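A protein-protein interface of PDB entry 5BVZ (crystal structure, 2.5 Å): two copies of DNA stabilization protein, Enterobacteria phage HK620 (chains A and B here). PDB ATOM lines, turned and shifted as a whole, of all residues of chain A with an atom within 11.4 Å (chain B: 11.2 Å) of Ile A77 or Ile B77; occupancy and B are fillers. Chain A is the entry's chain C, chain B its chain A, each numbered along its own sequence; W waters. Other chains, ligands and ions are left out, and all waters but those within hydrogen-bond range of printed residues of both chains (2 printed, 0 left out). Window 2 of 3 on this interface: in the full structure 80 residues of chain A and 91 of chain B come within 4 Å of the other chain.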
ATOM      1  N   GLN A  66      35.907   4.423 -40.252  1.00  0.00           N
ATOM      2  CA  GLN A  66      35.130   5.645 -40.095  1.00  0.00           C
ATOM      3  C   GLN A  66      33.678   5.327 -39.761  1.00  0.00           C
ATOM      4  O   GLN A  66      32.992   6.116 -39.108  1.00  0.00           O
ATOM      5  CB  GLN A  66      35.230   6.507 -41.356  1.00  0.00           C
ATOM      6  CG  GLN A  66      36.548   7.272 -41.460  1.00  0.00           C
ATOM      7  CD  GLN A  66      36.666   8.089 -42.734  1.00  0.00           C
ATOM      8  OE1 GLN A  66      35.968   7.833 -43.714  1.00  0.00           O
ATOM      9  NE2 GLN A  66      37.541   9.087 -42.720  1.00  0.00           N
ATOM     10  N   VAL A  68      32.717   2.755 -37.863  1.00  0.00           N
ATOM     11  CA  VAL A  68      32.724   2.459 -36.436  1.00  0.00           C
ATOM     12  C   VAL A  68      32.639   3.753 -35.643  1.00  0.00           C
ATOM     13  O   VAL A  68      31.875   3.858 -34.680  1.00  0.00           O
ATOM     14  CB  VAL A  68      33.987   1.680 -36.007  1.00  0.00           C
ATOM     15  CG1 VAL A  68      34.069   1.574 -34.489  1.00  0.00           C
ATOM     16  CG2 VAL A  68      34.004   0.299 -36.645  1.00  0.00           C
ATOM     17  N   GLU A  69      33.407   4.747 -36.073  1.00  0.00           N
ATOM     18  CA  GLU A  69      33.434   6.031 -35.392  1.00  0.00           C
ATOM     19  C   GLU A  69      32.094   6.752 -35.475  1.00  0.00           C
ATOM     20  O   GLU A  69      31.623   7.307 -34.488  1.00  0.00           O
ATOM     21  CB  GLU A  69      34.525   6.912 -36.004  1.00  0.00           C
ATOM     22  CG  GLU A  69      35.728   7.181 -35.125  1.00  0.00           C
ATOM     23  CD  GLU A  69      36.872   7.778 -35.919  1.00  0.00           C
ATOM     24  OE1 GLU A  69      36.802   7.749 -37.167  1.00  0.00           O
ATOM     25  OE2 GLU A  69      37.831   8.290 -35.304  1.00  0.00           O
ATOM     26  N   LEU A  70      31.467   6.704 -36.648  1.00  0.00           N
ATOM     27  CA  LEU A  70      30.161   7.326 -36.850  1.00  0.00           C
ATOM     28  C   LEU A  70      29.055   6.664 -36.023  1.00  0.00           C
ATOM     29  O   LEU A  70      28.173   7.346 -35.490  1.00  0.00           O
ATOM     30  CB  LEU A  70      29.794   7.299 -38.333  1.00  0.00           C
ATOM     31  CG  LEU A  70      30.512   8.355 -39.174  1.00  0.00           C
ATOM     32  CD1 LEU A  70      30.268   8.112 -40.657  1.00  0.00           C
ATOM     33  CD2 LEU A  70      30.102   9.772 -38.773  1.00  0.00           C
ATOM     34  N   ALA A  71      29.102   5.337 -35.928  1.00  0.00           N
ATOM     35  CA  ALA A  71      28.153   4.584 -35.115  1.00  0.00           C
ATOM     36  C   ALA A  71      28.334   4.952 -33.647  1.00  0.00           C
ATOM     37  O   ALA A  71      27.359   5.107 -32.909  1.00  0.00           O
ATOM     38  CB  ALA A  71      28.329   3.085 -35.325  1.00  0.00           C
ATOM     39  N   ASP A  72      29.593   5.063 -33.227  1.00  0.00           N
ATOM     40  CA  ASP A  72      29.918   5.469 -31.866  1.00  0.00           C
ATOM     41  C   ASP A  72      29.424   6.886 -31.580  1.00  0.00           C
ATOM     42  O   ASP A  72      28.815   7.141 -30.538  1.00  0.00           O
ATOM     43  CB  ASP A  72      31.431   5.385 -31.634  1.00  0.00           C
ATOM     44  CG  ASP A  72      31.860   6.000 -30.310  1.00  0.00           C
ATOM     45  OD1 ASP A  72      31.758   5.318 -29.269  1.00  0.00           O
ATOM     46  OD2 ASP A  72      32.306   7.167 -30.314  1.00  0.00           O
ATOM     47  N   HIS A  73      29.658   7.789 -32.529  1.00  0.00           N
ATOM     48  CA  HIS A  73      29.211   9.170 -32.407  1.00  0.00           C
ATOM     49  C   HIS A  73      27.687   9.248 -32.339  1.00  0.00           C
ATOM     50  O   HIS A  73      27.133  10.012 -31.546  1.00  0.00           O
ATOM     51  CB  HIS A  73      29.718  10.012 -33.586  1.00  0.00           C
ATOM     52  CG  HIS A  73      31.175  10.352 -33.504  1.00  0.00           C
ATOM     53  ND1 HIS A  73      31.775  11.235 -34.383  1.00  0.00           N
ATOM     54  CD2 HIS A  73      32.154   9.936 -32.673  1.00  0.00           C
ATOM     55  CE1 HIS A  73      33.060  11.345 -34.088  1.00  0.00           C
ATOM     56  NE2 HIS A  73      33.312  10.558 -33.048  1.00  0.00           N
ATOM     57  N   ASP A  74      27.023   8.457 -33.178  1.00  0.00           N
ATOM     58  CA  ASP A  74      25.562   8.435 -33.250  1.00  0.00           C
ATOM     59  C   ASP A  74      24.950   8.081 -31.899  1.00  0.00           C
ATOM     60  O   ASP A  74      24.030   8.748 -31.427  1.00  0.00           O
ATOM     61  CB  ASP A  74      25.091   7.430 -34.308  1.00  0.00           C
ATOM     62  CG  ASP A  74      23.587   7.459 -34.515  1.00  0.00           C
ATOM     63  OD1 ASP A  74      22.981   8.540 -34.353  1.00  0.00           O
ATOM     64  OD2 ASP A  74      23.006   6.392 -34.819  1.00  0.00           O
ATOM     65  N   ALA A  75      25.469   7.021 -31.289  1.00  0.00           N
ATOM     66  CA  ALA A  75      25.025   6.589 -29.972  1.00  0.00           C
ATOM     67  C   ALA A  75      25.322   7.652 -28.911  1.00  0.00           C
ATOM     68  O   ALA A  75      24.501   7.925 -28.036  1.00  0.00           O
ATOM     69  CB  ALA A  75      25.683   5.258 -29.603  1.00  0.00           C
ATOM     70  N   ARG A  76      26.504   8.249 -29.002  1.00  0.00           N
ATOM     71  CA  ARG A  76      26.938   9.252 -28.037  1.00  0.00           C
ATOM     72  C   ARG A  76      26.084  10.517 -28.111  1.00  0.00           C
ATOM     73  O   ARG A  76      25.661  11.038 -27.082  1.00  0.00           O
ATOM     74  CB  ARG A  76      28.417   9.558 -28.265  1.00  0.00           C
ATOM     75  CG  ARG A  76      29.343   8.473 -27.708  1.00  0.00           C
ATOM     76  CD  ARG A  76      30.807   8.753 -28.011  1.00  0.00           C
ATOM     77  NE  ARG A  76      31.263  10.063 -27.566  1.00  0.00           N
ATOM     78  CZ  ARG A  76      32.388  10.634 -27.984  1.00  0.00           C
ATOM     79  NH1 ARG A  76      33.161  10.007 -28.865  1.00  0.00           N
ATOM     80  NH2 ARG A  76      32.740  11.831 -27.534  1.00  0.00           N
ATOM     81  N   ILE A  77      25.795  10.990 -29.317  1.00  0.00           N
ATOM     82  CA  ILE A  77      24.937  12.163 -29.472  1.00  0.00           C
ATOM     83  C   ILE A  77      23.524  11.857 -28.957  1.00  0.00           C
ATOM     84  O   ILE A  77      22.934  12.654 -28.219  1.00  0.00           O
ATOM     85  CB  ILE A  77      24.878  12.634 -30.941  1.00  0.00           C
ATOM     86  CG1 ILE A  77      26.260  13.120 -31.393  1.00  0.00           C
ATOM     87  CG2 ILE A  77      23.847  13.746 -31.112  1.00  0.00           C
ATOM     88  CD1 ILE A  77      26.425  13.225 -32.900  1.00  0.00           C
ATOM     89  N   ALA A  78      23.008  10.687 -29.327  1.00  0.00           N
ATOM     90  CA  ALA A  78      21.690  10.240 -28.884  1.00  0.00           C
ATOM     91  C   ALA A  78      21.619  10.152 -27.362  1.00  0.00           C
ATOM     92  O   ALA A  78      20.625  10.552 -26.755  1.00  0.00           O
ATOM     93  CB  ALA A  78      21.349   8.895 -29.510  1.00  0.00           C
ATOM     94  N   ALA A  79      22.684   9.638 -26.749  1.00  0.00           N
ATOM     95  CA  ALA A  79      22.761   9.541 -25.294  1.00  0.00           C
ATOM     96  C   ALA A  79      22.730  10.930 -24.643  1.00  0.00           C
ATOM     97  O   ALA A  79      22.050  11.137 -23.637  1.00  0.00           O
ATOM     98  CB  ALA A  79      24.012   8.784 -24.882  1.00  0.00           C
ATOM     99  N   ASN A  80      23.473  11.875 -25.212  1.00  0.00           N
ATOM    100  CA  ASN A  80      23.453  13.253 -24.735  1.00  0.00           C
ATOM    101  C   ASN A  80      22.078  13.908 -24.838  1.00  0.00           C
ATOM    102  O   ASN A  80      21.623  14.574 -23.899  1.00  0.00           O
ATOM    103  CB  ASN A  80      24.465  14.094 -25.514  1.00  0.00           C
ATOM    104  CG  ASN A  80      25.878  13.900 -25.022  1.00  0.00           C
ATOM    105  OD1 ASN A  80      26.096  13.391 -23.928  1.00  0.00           O
ATOM    106  ND2 ASN A  80      26.852  14.295 -25.839  1.00  0.00           N
ATOM    107  N   THR A  81      21.429  13.717 -25.985  1.00  0.00           N
ATOM    108  CA  THR A  81      20.115  14.296 -26.240  1.00  0.00           C
ATOM    109  C   THR A  81      19.060  13.808 -25.257  1.00  0.00           C
ATOM    110  O   THR A  81      18.300  14.603 -24.701  1.00  0.00           O
ATOM    111  CB  THR A  81      19.638  13.978 -27.664  1.00  0.00           C
ATOM    112  OG1 THR A  81      20.596  14.465 -28.609  1.00  0.00           O
ATOM    113  CG2 THR A  81      18.284  14.621 -27.930  1.00  0.00           C
ATOM    114  N   LYS A  82      19.011  12.496 -25.055  1.00  0.00           N
ATOM    115  CA  LYS A  82      18.085  11.914 -24.099  1.00  0.00           C
ATOM    116  C   LYS A  82      18.391  12.422 -22.689  1.00  0.00           C
ATOM    117  O   LYS A  82      17.476  12.750 -21.924  1.00  0.00           O
ATOM    118  CB  LYS A  82      18.120  10.391 -24.156  1.00  0.00           C
ATOM    119  CG  LYS A  82      17.054   9.736 -23.296  1.00  0.00           C
ATOM    120  CD  LYS A  82      17.329   8.266 -23.098  1.00  0.00           C
ATOM    121  CE  LYS A  82      16.278   7.627 -22.211  1.00  0.00           C
ATOM    122  NZ  LYS A  82      14.911   8.095 -22.560  1.00  0.00           N
ATOM    123  N   ALA A  83      19.678  12.466 -22.344  1.00  0.00           N
ATOM    124  CA  ALA A  83      20.109  12.912 -21.019  1.00  0.00           C
ATOM    125  C   ALA A  83      19.644  14.341 -20.751  1.00  0.00           C
ATOM    126  O   ALA A  83      19.191  14.653 -19.651  1.00  0.00           O
ATOM    127  CB  ALA A  83      21.624  12.808 -20.879  1.00  0.00           C
ATOM    128  N   ILE A  84      19.765  15.196 -21.763  1.00  0.00           N
ATOM    129  CA  ILE A  84      19.304  16.577 -21.676  1.00  0.00           C
ATOM    130  C   ILE A  84      17.803  16.635 -21.367  1.00  0.00           C
ATOM    131  O   ILE A  84      17.358  17.412 -20.515  1.00  0.00           O
ATOM    132  CB  ILE A  84      19.592  17.342 -22.984  1.00  0.00           C
ATOM    133  CG1 ILE A  84      21.096  17.596 -23.135  1.00  0.00           C
ATOM    134  CG2 ILE A  84      18.848  18.662 -23.009  1.00  0.00           C
ATOM    135  CD1 ILE A  84      21.524  17.997 -24.532  1.00  0.00           C
ATOM    136  N   ASN A  85      17.032  15.794 -22.050  1.00  0.00           N
ATOM    137  CA  ASN A  85      15.592  15.730 -21.837  1.00  0.00           C
ATOM    138  C   ASN A  85      15.258  15.251 -20.429  1.00  0.00           C
ATOM    139  O   ASN A  85      14.285  15.706 -19.824  1.00  0.00           O
ATOM    140  CB  ASN A  85      14.935  14.816 -22.874  1.00  0.00           C
ATOM    141  CG  ASN A  85      15.067  15.348 -24.290  1.00  0.00           C
ATOM    142  OD1 ASN A  85      15.107  16.557 -24.507  1.00  0.00           O
ATOM    143  ND2 ASN A  85      15.137  14.444 -25.262  1.00  0.00           N
ATOM    144  N   ILE A  86      16.067  14.334 -19.910  1.00  0.00           N
ATOM    145  CA  ILE A  86      15.903  13.865 -18.541  1.00  0.00           C
ATOM    146  C   ILE A  86      16.182  15.002 -17.554  1.00  0.00           C
ATOM    147  O   ILE A  86      15.419  15.205 -16.601  1.00  0.00           O
ATOM    148  CB  ILE A  86      16.822  12.662 -18.234  1.00  0.00           C
ATOM    149  CG1 ILE A  86      16.399  11.445 -19.059  1.00  0.00           C
ATOM    150  CG2 ILE A  86      16.780  12.317 -16.756  1.00  0.00           C
ATOM    151  CD1 ILE A  86      17.293  10.234 -18.877  1.00  0.00           C
ATOM    152  N   ASP B  67      38.049  12.774 -41.456  1.00  0.00           N
ATOM    153  CA  ASP B  67      38.553  12.475 -40.119  1.00  0.00           C
ATOM    154  C   ASP B  67      38.775  13.726 -39.282  1.00  0.00           C
ATOM    155  O   ASP B  67      38.583  13.696 -38.068  1.00  0.00           O
ATOM    156  CB  ASP B  67      39.826  11.650 -40.184  1.00  0.00           C
ATOM    157  CG  ASP B  67      39.540  10.169 -40.250  1.00  0.00           C
ATOM    158  OD1 ASP B  67      38.367   9.773 -40.052  1.00  0.00           O
ATOM    159  OD2 ASP B  67      40.489   9.400 -40.473  1.00  0.00           O
ATOM    160  N   VAL B  68      39.174  14.817 -39.929  1.00  0.00           N
ATOM    161  CA  VAL B  68      39.275  16.095 -39.237  1.00  0.00           C
ATOM    162  C   VAL B  68      37.903  16.436 -38.671  1.00  0.00           C
ATOM    163  O   VAL B  68      37.782  16.871 -37.527  1.00  0.00           O
ATOM    164  CB  VAL B  68      39.761  17.232 -40.168  1.00  0.00           C
ATOM    165  CG1 VAL B  68      39.638  18.582 -39.481  1.00  0.00           C
ATOM    166  CG2 VAL B  68      41.193  16.977 -40.629  1.00  0.00           C
ATOM    167  N   GLU B  69      36.868  16.211 -39.475  1.00  0.00           N
ATOM    168  CA  GLU B  69      35.502  16.464 -39.046  1.00  0.00           C
ATOM    169  C   GLU B  69      35.130  15.514 -37.907  1.00  0.00           C
ATOM    170  O   GLU B  69      34.485  15.910 -36.942  1.00  0.00           O
ATOM    171  CB  GLU B  69      34.535  16.305 -40.226  1.00  0.00           C
ATOM    172  CG  GLU B  69      33.063  16.562 -39.900  1.00  0.00           C
ATOM    173  CD  GLU B  69      32.768  18.016 -39.532  1.00  0.00           C
ATOM    174  OE1 GLU B  69      33.651  18.884 -39.725  1.00  0.00           O
ATOM    175  OE2 GLU B  69      31.643  18.293 -39.059  1.00  0.00           O
ATOM    176  N   LEU B  70      35.579  14.268 -38.004  1.00  0.00           N
ATOM    177  CA  LEU B  70      35.330  13.301 -36.945  1.00  0.00           C
ATOM    178  C   LEU B  70      36.014  13.708 -35.645  1.00  0.00           C
ATOM    179  O   LEU B  70      35.454  13.525 -34.565  1.00  0.00           O
ATOM    180  CB  LEU B  70      35.776  11.908 -37.378  1.00  0.00           C
ATOM    181  CG  LEU B  70      34.751  11.269 -38.311  1.00  0.00           C
ATOM    182  CD1 LEU B  70      35.286   9.994 -38.944  1.00  0.00           C
ATOM    183  CD2 LEU B  70      33.466  10.995 -37.548  1.00  0.00           C
ATOM    184  N   ALA B  71      37.219  14.260 -35.747  1.00  0.00           N
ATOM    185  CA  ALA B  71      37.939  14.742 -34.568  1.00  0.00           C
ATOM    186  C   ALA B  71      37.201  15.902 -33.902  1.00  0.00           C
ATOM    187  O   ALA B  71      37.028  15.926 -32.681  1.00  0.00           O
ATOM    188  CB  ALA B  71      39.350  15.169 -34.945  1.00  0.00           C
ATOM    189  N   ASP B  72      36.739  16.841 -34.721  1.00  0.00           N
ATOM    190  CA  ASP B  72      35.995  17.994 -34.245  1.00  0.00           C
ATOM    191  C   ASP B  72      34.705  17.559 -33.555  1.00  0.00           C
ATOM    192  O   ASP B  72      34.350  18.079 -32.497  1.00  0.00           O
ATOM    193  CB  ASP B  72      35.679  18.936 -35.411  1.00  0.00           C
ATOM    194  CG  ASP B  72      34.738  20.067 -35.020  1.00  0.00           C
ATOM    195  OD1 ASP B  72      35.215  21.084 -34.473  1.00  0.00           O
ATOM    196  OD2 ASP B  72      33.516  19.934 -35.259  1.00  0.00           O
ATOM    197  N   HIS B  73      34.008  16.601 -34.159  1.00  0.00           N
ATOM    198  CA  HIS B  73      32.782  16.076 -33.570  1.00  0.00           C
ATOM    199  C   HIS B  73      33.028  15.378 -32.243  1.00  0.00           C
ATOM    200  O   HIS B  73      32.296  15.591 -31.281  1.00  0.00           O
ATOM    201  CB  HIS B  73      32.087  15.121 -34.536  1.00  0.00           C
ATOM    202  CG  HIS B  73      31.374  15.813 -35.650  1.00  0.00           C
ATOM    203  ND1 HIS B  73      30.536  15.155 -36.523  1.00  0.00           N
ATOM    204  CD2 HIS B  73      31.373  17.113 -36.037  1.00  0.00           C
ATOM    205  CE1 HIS B  73      30.044  16.017 -37.395  1.00  0.00           C
ATOM    206  NE2 HIS B  73      30.540  17.211 -37.123  1.00  0.00           N
ATOM    207  N   ASP B  74      34.073  14.564 -32.194  1.00  0.00           N
ATOM    208  CA  ASP B  74      34.402  13.815 -30.989  1.00  0.00           C
ATOM    209  C   ASP B  74      34.634  14.768 -29.812  1.00  0.00           C
ATOM    210  O   ASP B  74      34.084  14.575 -28.727  1.00  0.00           O
ATOM    211  CB  ASP B  74      35.633  12.932 -31.236  1.00  0.00           C
ATOM    212  CG  ASP B  74      35.956  12.036 -30.059  1.00  0.00           C
ATOM    213  OD1 ASP B  74      35.020  11.651 -29.328  1.00  0.00           O
ATOM    214  OD2 ASP B  74      37.143  11.705 -29.866  1.00  0.00           O
ATOM    215  N   ALA B  75      35.426  15.810 -30.049  1.00  0.00           N
ATOM    216  CA  ALA B  75      35.713  16.815 -29.033  1.00  0.00           C
ATOM    217  C   ALA B  75      34.445  17.548 -28.593  1.00  0.00           C
ATOM    218  O   ALA B  75      34.239  17.800 -27.409  1.00  0.00           O
ATOM    219  CB  ALA B  75      36.743  17.806 -29.547  1.00  0.00           C
ATOM    220  N   ARG B  76      33.603  17.885 -29.558  1.00  0.00           N
ATOM    221  CA  ARG B  76      32.363  18.598 -29.289  1.00  0.00           C
ATOM    222  C   ARG B  76      31.366  17.749 -28.489  1.00  0.00           C
ATOM    223  O   ARG B  76      30.747  18.231 -27.535  1.00  0.00           O
ATOM    224  CB  ARG B  76      31.749  19.042 -30.617  1.00  0.00           C
ATOM    225  CG  ARG B  76      32.440  20.247 -31.223  1.00  0.00           C
ATOM    226  CD  ARG B  76      31.836  20.621 -32.559  1.00  0.00           C
ATOM    227  NE  ARG B  76      30.400  20.855 -32.508  1.00  0.00           N
ATOM    228  CZ  ARG B  76      29.624  20.889 -33.587  1.00  0.00           C
ATOM    229  NH1 ARG B  76      30.151  20.686 -34.787  1.00  0.00           N
ATOM    230  NH2 ARG B  76      28.322  21.111 -33.470  1.00  0.00           N
ATOM    231  N   ILE B  77      31.226  16.483 -28.877  1.00  0.00           N
ATOM    232  CA  ILE B  77      30.343  15.554 -28.178  1.00  0.00           C
ATOM    233  C   ILE B  77      30.848  15.341 -26.752  1.00  0.00           C
ATOM    234  O   ILE B  77      30.067  15.343 -25.798  1.00  0.00           O
ATOM    235  CB  ILE B  77      30.246  14.196 -28.913  1.00  0.00           C
ATOM    236  CG1 ILE B  77      29.609  14.373 -30.295  1.00  0.00           C
ATOM    237  CG2 ILE B  77      29.450  13.188 -28.089  1.00  0.00           C
ATOM    238  CD1 ILE B  77      29.853  13.203 -31.235  1.00  0.00           C
ATOM    239  N   ALA B  78      32.161  15.170 -26.619  1.00  0.00           N
ATOM    240  CA  ALA B  78      32.801  14.983 -25.321  1.00  0.00           C
ATOM    241  C   ALA B  78      32.553  16.170 -24.399  1.00  0.00           C
ATOM    242  O   ALA B  78      32.304  15.997 -23.203  1.00  0.00           O
ATOM    243  CB  ALA B  78      34.303  14.761 -25.498  1.00  0.00           C
ATOM    244  N   ALA B  79      32.647  17.374 -24.956  1.00  0.00           N
ATOM    245  CA  ALA B  79      32.391  18.590 -24.193  1.00  0.00           C
ATOM    246  C   ALA B  79      30.927  18.658 -23.758  1.00  0.00           C
ATOM    247  O   ALA B  79      30.628  18.987 -22.611  1.00  0.00           O
ATOM    248  CB  ALA B  79      32.774  19.826 -25.006  1.00  0.00           C
ATOM    249  N   ASN B  80      30.016  18.335 -24.672  1.00  0.00           N
ATOM    250  CA  ASN B  80      28.593  18.308 -24.343  1.00  0.00           C
ATOM    251  C   ASN B  80      28.292  17.305 -23.237  1.00  0.00           C
ATOM    252  O   ASN B  80      27.520  17.590 -22.329  1.00  0.00           O
ATOM    253  CB  ASN B  80      27.744  17.996 -25.581  1.00  0.00           C
ATOM    254  CG  ASN B  80      27.564  19.208 -26.487  1.00  0.00           C
ATOM    255  OD1 ASN B  80      27.841  20.340 -26.091  1.00  0.00           O
ATOM    256  ND2 ASN B  80      27.054  18.980 -27.686  1.00  0.00           N
ATOM    257  N   THR B  81      28.881  16.119 -23.339  1.00  0.00           N
ATOM    258  CA  THR B  81      28.712  15.080 -22.328  1.00  0.00           C
ATOM    259  C   THR B  81      29.238  15.574 -20.986  1.00  0.00           C
ATOM    260  O   THR B  81      28.619  15.360 -19.940  1.00  0.00           O
ATOM    261  CB  THR B  81      29.428  13.764 -22.720  1.00  0.00           C
ATOM    262  OG1 THR B  81      28.906  13.289 -23.966  1.00  0.00           O
ATOM    263  CG2 THR B  81      29.225  12.695 -21.656  1.00  0.00           C
ATOM    264  N   LYS B  82      30.398  16.217 -21.020  1.00  0.00           N
ATOM    265  CA  LYS B  82      30.990  16.798 -19.821  1.00  0.00           C
ATOM    266  C   LYS B  82      30.060  17.798 -19.153  1.00  0.00           C
ATOM    267  O   LYS B  82      29.823  17.719 -17.951  1.00  0.00           O
ATOM    268  CB  LYS B  82      32.306  17.489 -20.185  1.00  0.00           C
ATOM    269  CG  LYS B  82      33.568  16.828 -19.673  1.00  0.00           C
ATOM    270  CD  LYS B  82      33.612  16.800 -18.158  1.00  0.00           C
ATOM    271  CE  LYS B  82      35.030  17.053 -17.682  1.00  0.00           C
ATOM    272  NZ  LYS B  82      35.135  17.124 -16.204  1.00  0.00           N
ATOM    273  N   ALA B  83      29.518  18.718 -19.947  1.00  0.00           N
ATOM    274  CA  ALA B  83      28.621  19.750 -19.436  1.00  0.00           C
ATOM    275  C   ALA B  83      27.369  19.138 -18.814  1.00  0.00           C
ATOM    276  O   ALA B  83      26.927  19.543 -17.743  1.00  0.00           O
ATOM    277  CB  ALA B  83      28.242  20.725 -20.544  1.00  0.00           C
ATOM    278  N   ILE B  84      26.817  18.144 -19.495  1.00  0.00           N
ATOM    279  CA  ILE B  84      25.629  17.446 -19.023  1.00  0.00           C
ATOM    280  C   ILE B  84      25.867  16.799 -17.660  1.00  0.00           C
ATOM    281  O   ILE B  84      25.025  16.896 -16.768  1.00  0.00           O
ATOM    282  CB  ILE B  84      25.176  16.386 -20.046  1.00  0.00           C
ATOM    283  CG1 ILE B  84      24.621  17.081 -21.293  1.00  0.00           C
ATOM    284  CG2 ILE B  84      24.125  15.469 -19.446  1.00  0.00           C
ATOM    285  CD1 ILE B  84      24.506  16.175 -22.495  1.00  0.00           C
ATOM    286  N   ASN B  85      27.014  16.149 -17.492  1.00  0.00           N
ATOM    287  CA  ASN B  85      27.337  15.552 -16.200  1.00  0.00           C
ATOM    288  C   ASN B  85      27.501  16.617 -15.119  1.00  0.00           C
ATOM    289  O   ASN B  85      27.105  16.407 -13.972  1.00  0.00           O
ATOM    290  CB  ASN B  85      28.603  14.693 -16.284  1.00  0.00           C
ATOM    291  CG  ASN B  85      28.421  13.465 -17.156  1.00  0.00           C
ATOM    292  OD1 ASN B  85      27.322  12.922 -17.250  1.00  0.00           O
ATOM    293  ND2 ASN B  85      29.504  13.006 -17.776  1.00  0.00           N
ATOM    294  N   ILE B  86      28.075  17.758 -15.494  1.00  0.00           N
ATOM    295  CA  ILE B  86      28.209  18.889 -14.583  1.00  0.00           C
ATOM    296  C   ILE B  86      26.854  19.484 -14.203  1.00  0.00           C
ATOM    297  O   ILE B  86      26.584  19.732 -13.024  1.00  0.00           O
ATOM    298  CB  ILE B  86      29.103  19.986 -15.197  1.00  0.00           C
ATOM    299  CG1 ILE B  86      30.539  19.472 -15.321  1.00  0.00           C
ATOM    300  CG2 ILE B  86      29.070  21.251 -14.351  1.00  0.00           C
ATOM    301  CD1 ILE B  86      31.484  20.441 -15.987  1.00  0.00           C
HETATM  302  O   HOH W   1      29.819  12.755 -36.253  1.00  0.00           O
HETATM  303  O   HOH W   2      30.962  12.158 -25.310  1.00  0.00           O
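OD1 of Asn A80 sits at hydrogen-bond distance from OG1 of Thr B81 (2.8 Å). OD1 of Asp B74 is in salt-bridge range of NH1 of Arg A76 (2.5 Å). O of Ile B77 sits at hydrogen-bond distance from ND2 of Asn A80. The side-chain amide nitrogen (NE2) of Gln A66 is in hydrogen-bond range of the side-chain carboxylate (OD1) of Asp B67.
The backbone carbonyl oxygen (O) of Thr B81 sits at hydrogen-bond distance from the side-chain amide nitrogen (ND2) of Asn B85 (3.3 Å). The backbone carbonyl oxygen (O) of Ile B77 is in hydrogen-bond range of the side-chain hydroxyl (OG1) of Thr B81 (3.0 Å). OE2 of Glu B69 lies within hydrogen-bond range of NE2 of His B73. O of Ile A77 sits at hydrogen-bond distance from OG1 of Thr A81, at 3.0 Å. The side-chain carboxylate (OD2) of Asp A72 lies within salt-bridge range of the guanidinium group (NH1) of Arg A76, 3.3 Å away.
Among the printed residues, merely in contact across the chains: Glu A69 with Leu B70 (3.2 Å), His A73 with Leu B70 (3.3 Å), Arg A76 with Ala B78 (3.5 Å), Asn A80 with Ile B84 (3.5 Å), Ile A77 with Ile B77 (3.6 Å), Arg A76 with Ile B77 (3.6 Å), Ile A84 with Ile B84 (3.7 Å), His A73 with Asp B74 (3.8 Å), Leu A70 with Leu B70 (3.8 Å), Asn A80 with Asn B80 (3.8 Å), Glu A69 with Asp B67 (3.9 Å), His A73 with Ile B77 (3.9 Å), His A73 with His B73 (3.9 Å), Gln A66 with Leu B70 (3.9 Å) and Ala A83 with Ile B84 (3.9 Å).
Of chain B, only Ile B77 (3.6 Å) comes within 4 Å of Ile A77. Of chain A, only His A73, Arg A76, Ile A77 and Asn A80 come within 4 Å of Ile B77. His A73 touches four residues of chain B. Ala A75 touches none of the printed residues of chain B. No residue of chain B comes within 4 Å of Ala A79. No residue of chain B comes within 4 Å of Thr A81. Of chain A, only His A73 comes within 4 Å of His B73. No residue of chain A comes within 4 Å of Arg B76. Ala B78 touches just one residue of chain A: Arg A76 (3.5 Å). No residue of chain A comes within 4 Å of Ala B79. Asn B80 touches just one residue of chain A: Asn A80. Thr B81 touches just one residue of chain A: Asn A80. Printed residues of chain A within 4 Å of Asp B74: His A73 and Arg A76. Printed residues of chain B within 4 Å of Leu A70: Leu B70. Of the printed residues of chain A, Ile B84 touches Asn A80, Ala A83 and Ile A84.
Of the 20 printed residues of chain B, 9 touch a printed residue of chain A. Hydrophobic or aromatic side chains of chain B within 4 Å of the printed part of chain A: Leu B70, His B73, Ile B77, Ala B78 and Ile B84. Of the 20 printed residues of chain A, 9 touch a printed residue of chain B. Hydrophobic or aromatic side chains of chain A that line the printed part of chain B: Leu A70, His A73, Ile A77, Ala A83 and Ile A84.
Ile B77 touches its own counterpart, Ile A77. Asn A80 touches Ile B77, but with the chains exchanged Ile A77 does not touch Asn B80 (7.0 Å). Asn A80 touches Ile B84, but with the chains exchanged Ile A84 does not touch Asn B80 (6.3 Å). Ile B84 touches its own counterpart, Ile A84. 19 positions are printed for both chains.
Water W1 lies within hydrogen-bond range of ND1 of His B73 and ND1 of His A73. Water W2 lies within hydrogen-bond range of the side-chain hydroxyl (OG1) of Thr B81 (2.7 Å), the guanidinium group (NH2) of Arg A76 (2.9 Å), the backbone carbonyl oxygen (O) of Ile B77 (3.3 Å) and the backbone NH (N) of Ala B78 (3.5 Å).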
